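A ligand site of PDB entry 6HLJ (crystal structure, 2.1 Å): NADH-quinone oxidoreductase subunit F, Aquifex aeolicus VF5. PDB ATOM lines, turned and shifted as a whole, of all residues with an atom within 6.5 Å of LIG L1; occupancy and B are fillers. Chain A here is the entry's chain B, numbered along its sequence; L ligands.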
ATOM      1  N   ILE A 181      23.273 -18.232  32.088  1.00  0.00           N
ATOM      2  CA  ILE A 181      22.657 -18.354  30.774  1.00  0.00           C
ATOM      3  C   ILE A 181      21.168 -18.643  30.876  1.00  0.00           C
ATOM      4  O   ILE A 181      20.432 -18.321  29.954  1.00  0.00           O
ATOM      5  CB  ILE A 181      23.422 -19.385  29.878  1.00  0.00           C
ATOM      6  CG1 ILE A 181      23.119 -19.168  28.394  1.00  0.00           C
ATOM      7  CG2 ILE A 181      23.171 -20.852  30.297  1.00  0.00           C
ATOM      8  CD1 ILE A 181      23.277 -17.718  27.872  1.00  0.00           C
ATOM      9  N   GLU A 184      18.657 -16.037  29.881  1.00  0.00           N
ATOM     10  CA  GLU A 184      18.366 -15.827  28.461  1.00  0.00           C
ATOM     11  C   GLU A 184      17.006 -16.464  28.245  1.00  0.00           C
ATOM     12  O   GLU A 184      16.785 -17.592  28.700  1.00  0.00           O
ATOM     13  CB  GLU A 184      19.457 -16.477  27.559  1.00  0.00           C
ATOM     14  CG  GLU A 184      19.465 -15.934  26.145  1.00  0.00           C
ATOM     15  CD  GLU A 184      18.472 -16.554  25.185  1.00  0.00           C
ATOM     16  OE1 GLU A 184      17.992 -17.681  25.468  1.00  0.00           O
ATOM     17  OE2 GLU A 184      18.220 -15.947  24.119  1.00  0.00           O
ATOM     18  N   HIS A 198      20.240 -24.328  27.325  1.00  0.00           N
ATOM     19  CA  HIS A 198      20.890 -23.945  26.086  1.00  0.00           C
ATOM     20  C   HIS A 198      20.002 -23.011  25.297  1.00  0.00           C
ATOM     21  O   HIS A 198      18.919 -23.438  24.881  1.00  0.00           O
ATOM     22  CB  HIS A 198      21.251 -25.190  25.231  1.00  0.00           C
ATOM     23  CG  HIS A 198      22.379 -26.009  25.784  1.00  0.00           C
ATOM     24  ND1 HIS A 198      22.563 -27.320  25.402  1.00  0.00           N
ATOM     25  CD2 HIS A 198      23.366 -25.683  26.648  1.00  0.00           C
ATOM     26  CE1 HIS A 198      23.634 -27.744  26.055  1.00  0.00           C
ATOM     27  NE2 HIS A 198      24.160 -26.796  26.810  1.00  0.00           N
ATOM     28  N   PRO A 199      20.452 -21.763  25.004  1.00  0.00           N
ATOM     29  CA  PRO A 199      19.640 -20.875  24.163  1.00  0.00           C
ATOM     30  C   PRO A 199      19.261 -21.491  22.814  1.00  0.00           C
ATOM     31  O   PRO A 199      20.019 -22.315  22.266  1.00  0.00           O
ATOM     32  CB  PRO A 199      20.549 -19.666  23.959  1.00  0.00           C
ATOM     33  CG  PRO A 199      21.388 -19.634  25.204  1.00  0.00           C
ATOM     34  CD  PRO A 199      21.680 -21.085  25.456  1.00  0.00           C
ATOM     35  N   ARG A 200      18.073 -21.142  22.297  1.00  0.00           N
ATOM     36  CA  ARG A 200      17.604 -21.645  20.999  1.00  0.00           C
ATOM     37  C   ARG A 200      17.947 -20.619  19.944  1.00  0.00           C
ATOM     38  O   ARG A 200      17.979 -19.421  20.220  1.00  0.00           O
ATOM     39  CB  ARG A 200      16.079 -21.793  20.994  1.00  0.00           C
ATOM     40  CG  ARG A 200      15.487 -22.796  21.960  1.00  0.00           C
ATOM     41  CD  ARG A 200      14.006 -22.578  22.092  1.00  0.00           C
ATOM     42  NE  ARG A 200      13.394 -23.619  22.931  1.00  0.00           N
ATOM     43  CZ  ARG A 200      12.106 -23.721  23.197  1.00  0.00           C
ATOM     44  NH1 ARG A 200      11.241 -22.852  22.691  1.00  0.00           N
ATOM     45  NH2 ARG A 200      11.652 -24.711  23.955  1.00  0.00           N
ATOM     46  N   GLU A 345      30.405 -18.701  32.418  1.00  0.00           N
ATOM     47  CA  GLU A 345      29.001 -18.701  32.011  1.00  0.00           C
ATOM     48  C   GLU A 345      28.673 -19.073  30.559  1.00  0.00           C
ATOM     49  O   GLU A 345      27.490 -19.335  30.285  1.00  0.00           O
ATOM     50  CB  GLU A 345      28.334 -17.356  32.362  1.00  0.00           C
ATOM     51  CG  GLU A 345      28.331 -17.048  33.855  1.00  0.00           C
ATOM     52  CD  GLU A 345      27.883 -18.129  34.826  1.00  0.00           C
ATOM     53  OE1 GLU A 345      27.037 -18.981  34.480  1.00  0.00           O
ATOM     54  OE2 GLU A 345      28.310 -18.039  35.993  1.00  0.00           O
ATOM     55  N   THR A 346      29.628 -19.072  29.619  1.00  0.00           N
ATOM     56  CA  THR A 346      29.287 -19.476  28.240  1.00  0.00           C
ATOM     57  C   THR A 346      28.715 -20.917  28.258  1.00  0.00           C
ATOM     58  O   THR A 346      29.252 -21.763  28.959  1.00  0.00           O
ATOM     59  CB  THR A 346      30.502 -19.362  27.267  1.00  0.00           C
ATOM     60  OG1 THR A 346      30.131 -19.898  25.990  1.00  0.00           O
ATOM     61  CG2 THR A 346      31.761 -20.080  27.785  1.00  0.00           C
ATOM     62  N   CYS A 347      27.601 -21.169  27.546  1.00  0.00           N
ATOM     63  CA  CYS A 347      27.034 -22.517  27.514  1.00  0.00           C
ATOM     64  C   CYS A 347      27.825 -23.451  26.599  1.00  0.00           C
ATOM     65  O   CYS A 347      27.662 -24.663  26.709  1.00  0.00           O
ATOM     66  CB  CYS A 347      25.553 -22.519  27.194  1.00  0.00           C
ATOM     67  SG  CYS A 347      25.188 -22.310  25.444  1.00  0.00           S
ATOM     68  N   GLY A 348      28.650 -22.884  25.721  1.00  0.00           N
ATOM     69  CA  GLY A 348      29.549 -23.623  24.835  1.00  0.00           C
ATOM     70  C   GLY A 348      29.008 -24.111  23.509  1.00  0.00           C
ATOM     71  O   GLY A 348      29.720 -24.777  22.769  1.00  0.00           O
ATOM     72  N   GLN A 349      27.743 -23.797  23.178  1.00  0.00           N
ATOM     73  CA  GLN A 349      27.122 -24.242  21.916  1.00  0.00           C
ATOM     74  C   GLN A 349      27.809 -23.689  20.676  1.00  0.00           C
ATOM     75  O   GLN A 349      27.807 -24.323  19.622  1.00  0.00           O
ATOM     76  CB  GLN A 349      25.667 -23.774  21.853  1.00  0.00           C
ATOM     77  CG  GLN A 349      24.639 -24.670  22.484  1.00  0.00           C
ATOM     78  CD  GLN A 349      23.273 -24.104  22.152  1.00  0.00           C
ATOM     79  OE1 GLN A 349      22.646 -24.507  21.176  1.00  0.00           O
ATOM     80  NE2 GLN A 349      22.842 -23.066  22.883  1.00  0.00           N
ATOM     81  N   CYS A 350      28.253 -22.421  20.780  1.00  0.00           N
ATOM     82  CA  CYS A 350      28.859 -21.692  19.676  1.00  0.00           C
ATOM     83  C   CYS A 350      30.379 -21.708  19.907  1.00  0.00           C
ATOM     84  O   CYS A 350      30.826 -21.492  21.028  1.00  0.00           O
ATOM     85  CB  CYS A 350      28.305 -20.263  19.588  1.00  0.00           C
ATOM     86  SG  CYS A 350      26.494 -20.141  19.800  1.00  0.00           S
ATOM     87  N   THR A 351      31.146 -22.025  18.865  1.00  0.00           N
ATOM     88  CA  THR A 351      32.597 -22.183  18.940  1.00  0.00           C
ATOM     89  C   THR A 351      33.303 -20.848  19.260  1.00  0.00           C
ATOM     90  O   THR A 351      34.051 -20.833  20.234  1.00  0.00           O
ATOM     91  CB  THR A 351      33.137 -22.910  17.674  1.00  0.00           C
ATOM     92  OG1 THR A 351      32.667 -24.257  17.728  1.00  0.00           O
ATOM     93  CG2 THR A 351      34.662 -22.920  17.582  1.00  0.00           C
ATOM     94  N   CYS A 353      32.233 -18.294  20.825  1.00  0.00           N
ATOM     95  CA  CYS A 353      31.848 -17.958  22.184  1.00  0.00           C
ATOM     96  C   CYS A 353      32.538 -18.899  23.171  1.00  0.00           C
ATOM     97  O   CYS A 353      33.173 -18.426  24.117  1.00  0.00           O
ATOM     98  CB  CYS A 353      30.336 -17.947  22.380  1.00  0.00           C
ATOM     99  SG  CYS A 353      29.823 -17.495  24.059  1.00  0.00           S
ATOM    100  N   ARG A 354      32.433 -20.231  22.929  1.00  0.00           N
ATOM    101  CA  ARG A 354      33.026 -21.239  23.801  1.00  0.00           C
ATOM    102  C   ARG A 354      34.522 -21.032  23.983  1.00  0.00           C
ATOM    103  O   ARG A 354      34.999 -20.930  25.108  1.00  0.00           O
ATOM    104  CB  ARG A 354      32.741 -22.641  23.278  1.00  0.00           C
ATOM    105  CG  ARG A 354      33.393 -23.796  24.052  1.00  0.00           C
ATOM    106  CD  ARG A 354      33.093 -25.176  23.422  1.00  0.00           C
ATOM    107  NE  ARG A 354      33.791 -25.365  22.145  1.00  0.00           N
ATOM    108  CZ  ARG A 354      33.201 -25.330  20.953  1.00  0.00           C
ATOM    109  NH1 ARG A 354      31.885 -25.117  20.867  1.00  0.00           N
ATOM    110  NH2 ARG A 354      33.911 -25.501  19.844  1.00  0.00           N
ATOM    111  N   CYS A 357      35.493 -17.027  25.126  1.00  0.00           N
ATOM    112  CA  CYS A 357      35.302 -16.708  26.549  1.00  0.00           C
ATOM    113  C   CYS A 357      36.395 -17.354  27.388  1.00  0.00           C
ATOM    114  O   CYS A 357      36.880 -16.732  28.333  1.00  0.00           O
ATOM    115  CB  CYS A 357      33.918 -17.085  27.057  1.00  0.00           C
ATOM    116  SG  CYS A 357      32.579 -16.039  26.422  1.00  0.00           S
ATOM    117  N   ILE A 387      34.660 -13.005  19.865  1.00  0.00           N
ATOM    118  CA  ILE A 387      33.814 -13.922  20.646  1.00  0.00           C
ATOM    119  C   ILE A 387      32.422 -13.993  19.948  1.00  0.00           C
ATOM    120  O   ILE A 387      31.753 -15.048  19.944  1.00  0.00           O
ATOM    121  CB  ILE A 387      33.724 -13.468  22.136  1.00  0.00           C
ATOM    122  CG1 ILE A 387      35.134 -13.460  22.821  1.00  0.00           C
ATOM    123  CG2 ILE A 387      32.791 -14.371  22.921  1.00  0.00           C
ATOM    124  CD1 ILE A 387      35.213 -12.686  24.179  1.00  0.00           C
ATOM    125  N   GLN A 388      31.999 -12.872  19.346  1.00  0.00           N
ATOM    126  CA  GLN A 388      30.662 -12.704  18.736  1.00  0.00           C
ATOM    127  C   GLN A 388      30.376 -13.575  17.492  1.00  0.00           C
ATOM    128  O   GLN A 388      29.243 -14.034  17.395  1.00  0.00           O
ATOM    129  CB  GLN A 388      30.412 -11.221  18.406  1.00  0.00           C
ATOM    130  CG  GLN A 388      29.049 -10.905  17.768  1.00  0.00           C
ATOM    131  CD  GLN A 388      28.538  -9.485  18.035  1.00  0.00           C
ATOM    132  OE1 GLN A 388      27.356  -9.186  17.791  1.00  0.00           O
ATOM    133  NE2 GLN A 388      29.377  -8.585  18.555  1.00  0.00           N
ATOM    134  N   THR A 390      29.034 -16.039  14.757  1.00  0.00           N
ATOM    135  CA  THR A 390      28.150 -17.214  14.725  1.00  0.00           C
ATOM    136  C   THR A 390      27.275 -17.409  15.990  1.00  0.00           C
ATOM    137  O   THR A 390      26.472 -18.353  15.998  1.00  0.00           O
ATOM    138  CB  THR A 390      28.909 -18.544  14.400  1.00  0.00           C
ATOM    139  OG1 THR A 390      29.527 -19.023  15.593  1.00  0.00           O
ATOM    140  CG2 THR A 390      29.917 -18.416  13.260  1.00  0.00           C
ATOM    141  N   SER A 391      27.430 -16.553  17.048  1.00  0.00           N
ATOM    142  CA  SER A 391      26.695 -16.633  18.322  1.00  0.00           C
ATOM    143  C   SER A 391      25.191 -16.590  18.131  1.00  0.00           C
ATOM    144  O   SER A 391      24.692 -15.838  17.304  1.00  0.00           O
ATOM    145  CB  SER A 391      27.126 -15.516  19.282  1.00  0.00           C
ATOM    146  OG  SER A 391      26.925 -14.238  18.702  1.00  0.00           O
ATOM    147  N   ILE A 392      24.467 -17.435  18.877  1.00  0.00           N
ATOM    148  CA  ILE A 392      23.016 -17.500  18.738  1.00  0.00           C
ATOM    149  C   ILE A 392      22.296 -16.784  19.894  1.00  0.00           C
ATOM    150  O   ILE A 392      21.086 -16.802  19.907  1.00  0.00           O
ATOM    151  CB  ILE A 392      22.472 -18.912  18.466  1.00  0.00           C
ATOM    152  CG1 ILE A 392      22.754 -19.903  19.614  1.00  0.00           C
ATOM    153  CG2 ILE A 392      23.002 -19.416  17.118  1.00  0.00           C
ATOM    154  CD1 ILE A 392      22.266 -21.347  19.371  1.00  0.00           C
ATOM    155  N   CYS A 393      23.030 -16.177  20.861  1.00  0.00           N
ATOM    156  CA  CYS A 393      22.422 -15.420  21.965  1.00  0.00           C
ATOM    157  C   CYS A 393      23.296 -14.197  22.338  1.00  0.00           C
ATOM    158  O   CYS A 393      24.394 -14.056  21.807  1.00  0.00           O
ATOM    159  CB  CYS A 393      22.064 -16.297  23.158  1.00  0.00           C
ATOM    160  SG  CYS A 393      23.292 -16.345  24.506  1.00  0.00           S
ATOM    161  N   GLY A 394      22.740 -13.314  23.164  1.00  0.00           N
ATOM    162  CA  GLY A 394      23.364 -12.066  23.584  1.00  0.00           C
ATOM    163  C   GLY A 394      24.686 -12.184  24.328  1.00  0.00           C
ATOM    164  O   GLY A 394      25.474 -11.249  24.282  1.00  0.00           O
ATOM    165  N   LEU A 395      24.926 -13.305  25.027  1.00  0.00           N
ATOM    166  CA  LEU A 395      26.186 -13.517  25.754  1.00  0.00           C
ATOM    167  C   LEU A 395      27.461 -13.416  24.860  1.00  0.00           C
ATOM    168  O   LEU A 395      28.385 -12.666  25.198  1.00  0.00           O
ATOM    169  CB  LEU A 395      26.179 -14.825  26.553  1.00  0.00           C
ATOM    170  CG  LEU A 395      27.303 -14.997  27.607  1.00  0.00           C
ATOM    171  CD1 LEU A 395      26.819 -15.875  28.748  1.00  0.00           C
ATOM    172  CD2 LEU A 395      28.593 -15.574  26.969  1.00  0.00           C
ATOM    173  N   GLY A 396      27.473 -14.124  23.736  1.00  0.00           N
ATOM    174  CA  GLY A 396      28.624 -14.081  22.833  1.00  0.00           C
ATOM    175  C   GLY A 396      28.853 -12.696  22.270  1.00  0.00           C
ATOM    176  O   GLY A 396      30.003 -12.254  22.134  1.00  0.00           O
ATOM    177  N   ALA A 397      27.744 -11.968  21.988  1.00  0.00           N
ATOM    178  CA  ALA A 397      27.806 -10.616  21.421  1.00  0.00           C
ATOM    179  C   ALA A 397      28.384  -9.585  22.392  1.00  0.00           C
ATOM    180  O   ALA A 397      28.902  -8.561  21.944  1.00  0.00           O
ATOM    181  CB  ALA A 397      26.409 -10.177  20.970  1.00  0.00           C
HETATM  182 FE1  LIG L   1      25.879 -20.353  24.517  1.00  0.00          FE
HETATM  183 FE2  LIG L   1      27.648 -18.308  23.993  1.00  0.00          FE
HETATM  184 FE3  LIG L   1      24.961 -17.857  23.799  1.00  0.00          FE
HETATM  185 FE4  LIG L   1      26.206 -19.433  21.939  1.00  0.00          FE
HETATM  186  S1  LIG L   1      26.522 -17.176  22.315  1.00  0.00           S
HETATM  187  S2  LIG L   1      24.226 -19.876  22.959  1.00  0.00           S
HETATM  188  S3  LIG L   1      27.804 -20.487  23.278  1.00  0.00           S
HETATM  189  S4  LIG L   1      26.177 -18.424  25.690  1.00  0.00           S
HETATM  190  N1  LG2 L   2      16.461 -11.078  31.794  1.00  0.00           N
HETATM  191  C1  LG2 L   2      16.030 -11.108  33.076  1.00  0.00           C
HETATM  192  O1  LG2 L   2      14.890 -10.736  33.355  1.00  0.00           O
HETATM  193  N2  LG2 L   2      16.840 -11.657  34.079  1.00  0.00           N
HETATM  194  C2  LG2 L   2      18.090 -12.235  33.884  1.00  0.00           C
HETATM  195  O2  LG2 L   2      18.687 -12.746  34.836  1.00  0.00           O
HETATM  196  C3  LG2 L   2      18.532 -12.216  32.482  1.00  0.00           C
HETATM  197  N3  LG2 L   2      19.683 -12.763  32.190  1.00  0.00           N
HETATM  198  C4  LG2 L   2      20.071 -12.783  30.846  1.00  0.00           C
HETATM  199  C5  LG2 L   2      21.269 -13.410  30.502  1.00  0.00           C
HETATM  200  C6  LG2 L   2      21.698 -13.471  29.179  1.00  0.00           C
HETATM  201  C7  LG2 L   2      22.993 -14.172  28.854  1.00  0.00           C
HETATM  202  C8  LG2 L   2      20.907 -12.879  28.160  1.00  0.00           C
HETATM  203  C9  LG2 L   2      21.370 -12.823  26.720  1.00  0.00           C
HETATM  204  C10 LG2 L   2      19.694 -12.269  28.504  1.00  0.00           C
HETATM  205  C11 LG2 L   2      19.279 -12.207  29.824  1.00  0.00           C
HETATM  206  N4  LG2 L   2      18.045 -11.609  30.204  1.00  0.00           N
HETATM  207  C12 LG2 L   2      17.643 -11.606  31.517  1.00  0.00           C
HETATM  208  C13 LG2 L   2      17.166 -11.012  29.178  1.00  0.00           C
HETATM  209  C14 LG2 L   2      16.052 -11.966  28.759  1.00  0.00           C
HETATM  210  O3  LG2 L   2      16.509 -12.837  27.726  1.00  0.00           O
HETATM  211  C15 LG2 L   2      14.812 -11.196  28.296  1.00  0.00           C
HETATM  212  O4  LG2 L   2      15.217 -10.130  27.436  1.00  0.00           O
HETATM  213  C16 LG2 L   2      13.904 -10.616  29.384  1.00  0.00           C
HETATM  214  O5  LG2 L   2      13.699 -11.527  30.478  1.00  0.00           O
HETATM  215  C17 LG2 L   2      12.570 -10.199  28.822  1.00  0.00           C
HETATM  216  O6  LG2 L   2      11.853  -9.449  29.818  1.00  0.00           O
HETATM  217  P1  LG2 L   2      11.709  -7.850  29.789  1.00  0.00           P
HETATM  218  O7  LG2 L   2      13.018  -7.145  30.001  1.00  0.00           O
HETATM  219  O8  LG2 L   2      11.130  -7.491  28.366  1.00  0.00           O
HETATM  220  O9  LG2 L   2      10.696  -7.539  30.829  1.00  0.00           O
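Ile 181 touches LIG L1 (CD1 to S4, 3.7 Å).
CG of Pro 199 touches S2 of LIG L1 (3.6 Å).
Ser 391 touches LIG L1.
CG1 of Ile 392 touches S2 of LIG L1 (3.7 Å).
Leu 395 touches LIG L1 (CB to S4, 3.7 Å).
Hydrophobic or aromatic side chains within 4 Å of LIG L1: Ile 181, Pro 199, Ile 392 and Leu 395.
The backbone NH of Ile 392 lies close to the side-chain sulfur of Cys 350.
The side-chain sulfur (SG) of Cys 347 sits close to the side-chain amide nitrogen (NE2) of Gln 349 (3.6 Å).
The side-chain sulfur (SG) of Cys 353 sits close to the side-chain hydroxyl (OG1) of Thr 346.
O of Ile 387 is in hydrogen-bond range of N of Cys 353 (3.4 Å).
The backbone NH of Gln 388 sits at hydrogen-bond distance from the backbone carbonyl oxygen of Gly 396 (3.5 Å).
OG of Ser 391 sits at hydrogen-bond distance from O of Gln 388, 2.7 Å away.
The side-chain hydroxyl (OG1) of Thr 346 lies close to the backbone NH (N) of Gly 348 (3.3 Å).
The guanidinium group (NH1) of Arg 354 lies within hydrogen-bond range of the backbone carbonyl oxygen (O) of Gly 348 (2.9 Å).
The backbone NH (N) of Cys 350 sits close to a sulfur (S3) of LIG L1 (3.2 Å).
The side-chain sulfur (SG) of Cys 350 binds an iron atom (FE4) of LIG L1 (2.3 Å).
A sulfur (S4) of LIG L1 sits close to the backbone NH (N) of Cys 347 (3.6 Å).
SG of Cys 347 is bound to FE1 of LIG L1.
FE2 of LIG L1 is bound by SG of Cys 353, at 2.3 Å.
The side-chain sulfur (SG) of Cys 393 binds an iron atom (FE3) of LIG L1, at 2.4 Å.
S3 of LIG L1 lies close to N of Gln 349.
The side-chain amide nitrogen (NE2) of Gln 349 lies close to a sulfur (S2) of LIG L1.
A sulfur (S1) of LIG L1 sits close to the backbone NH (N) of Gly 396 (3.5 Å).
A sulfur (S3) of LIG L1 sits close to the backbone NH (N) of Gly 348, 3.5 Å away.
OG1 of Thr 346 sits close to S3 of LIG L1, at 3.6 Å.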
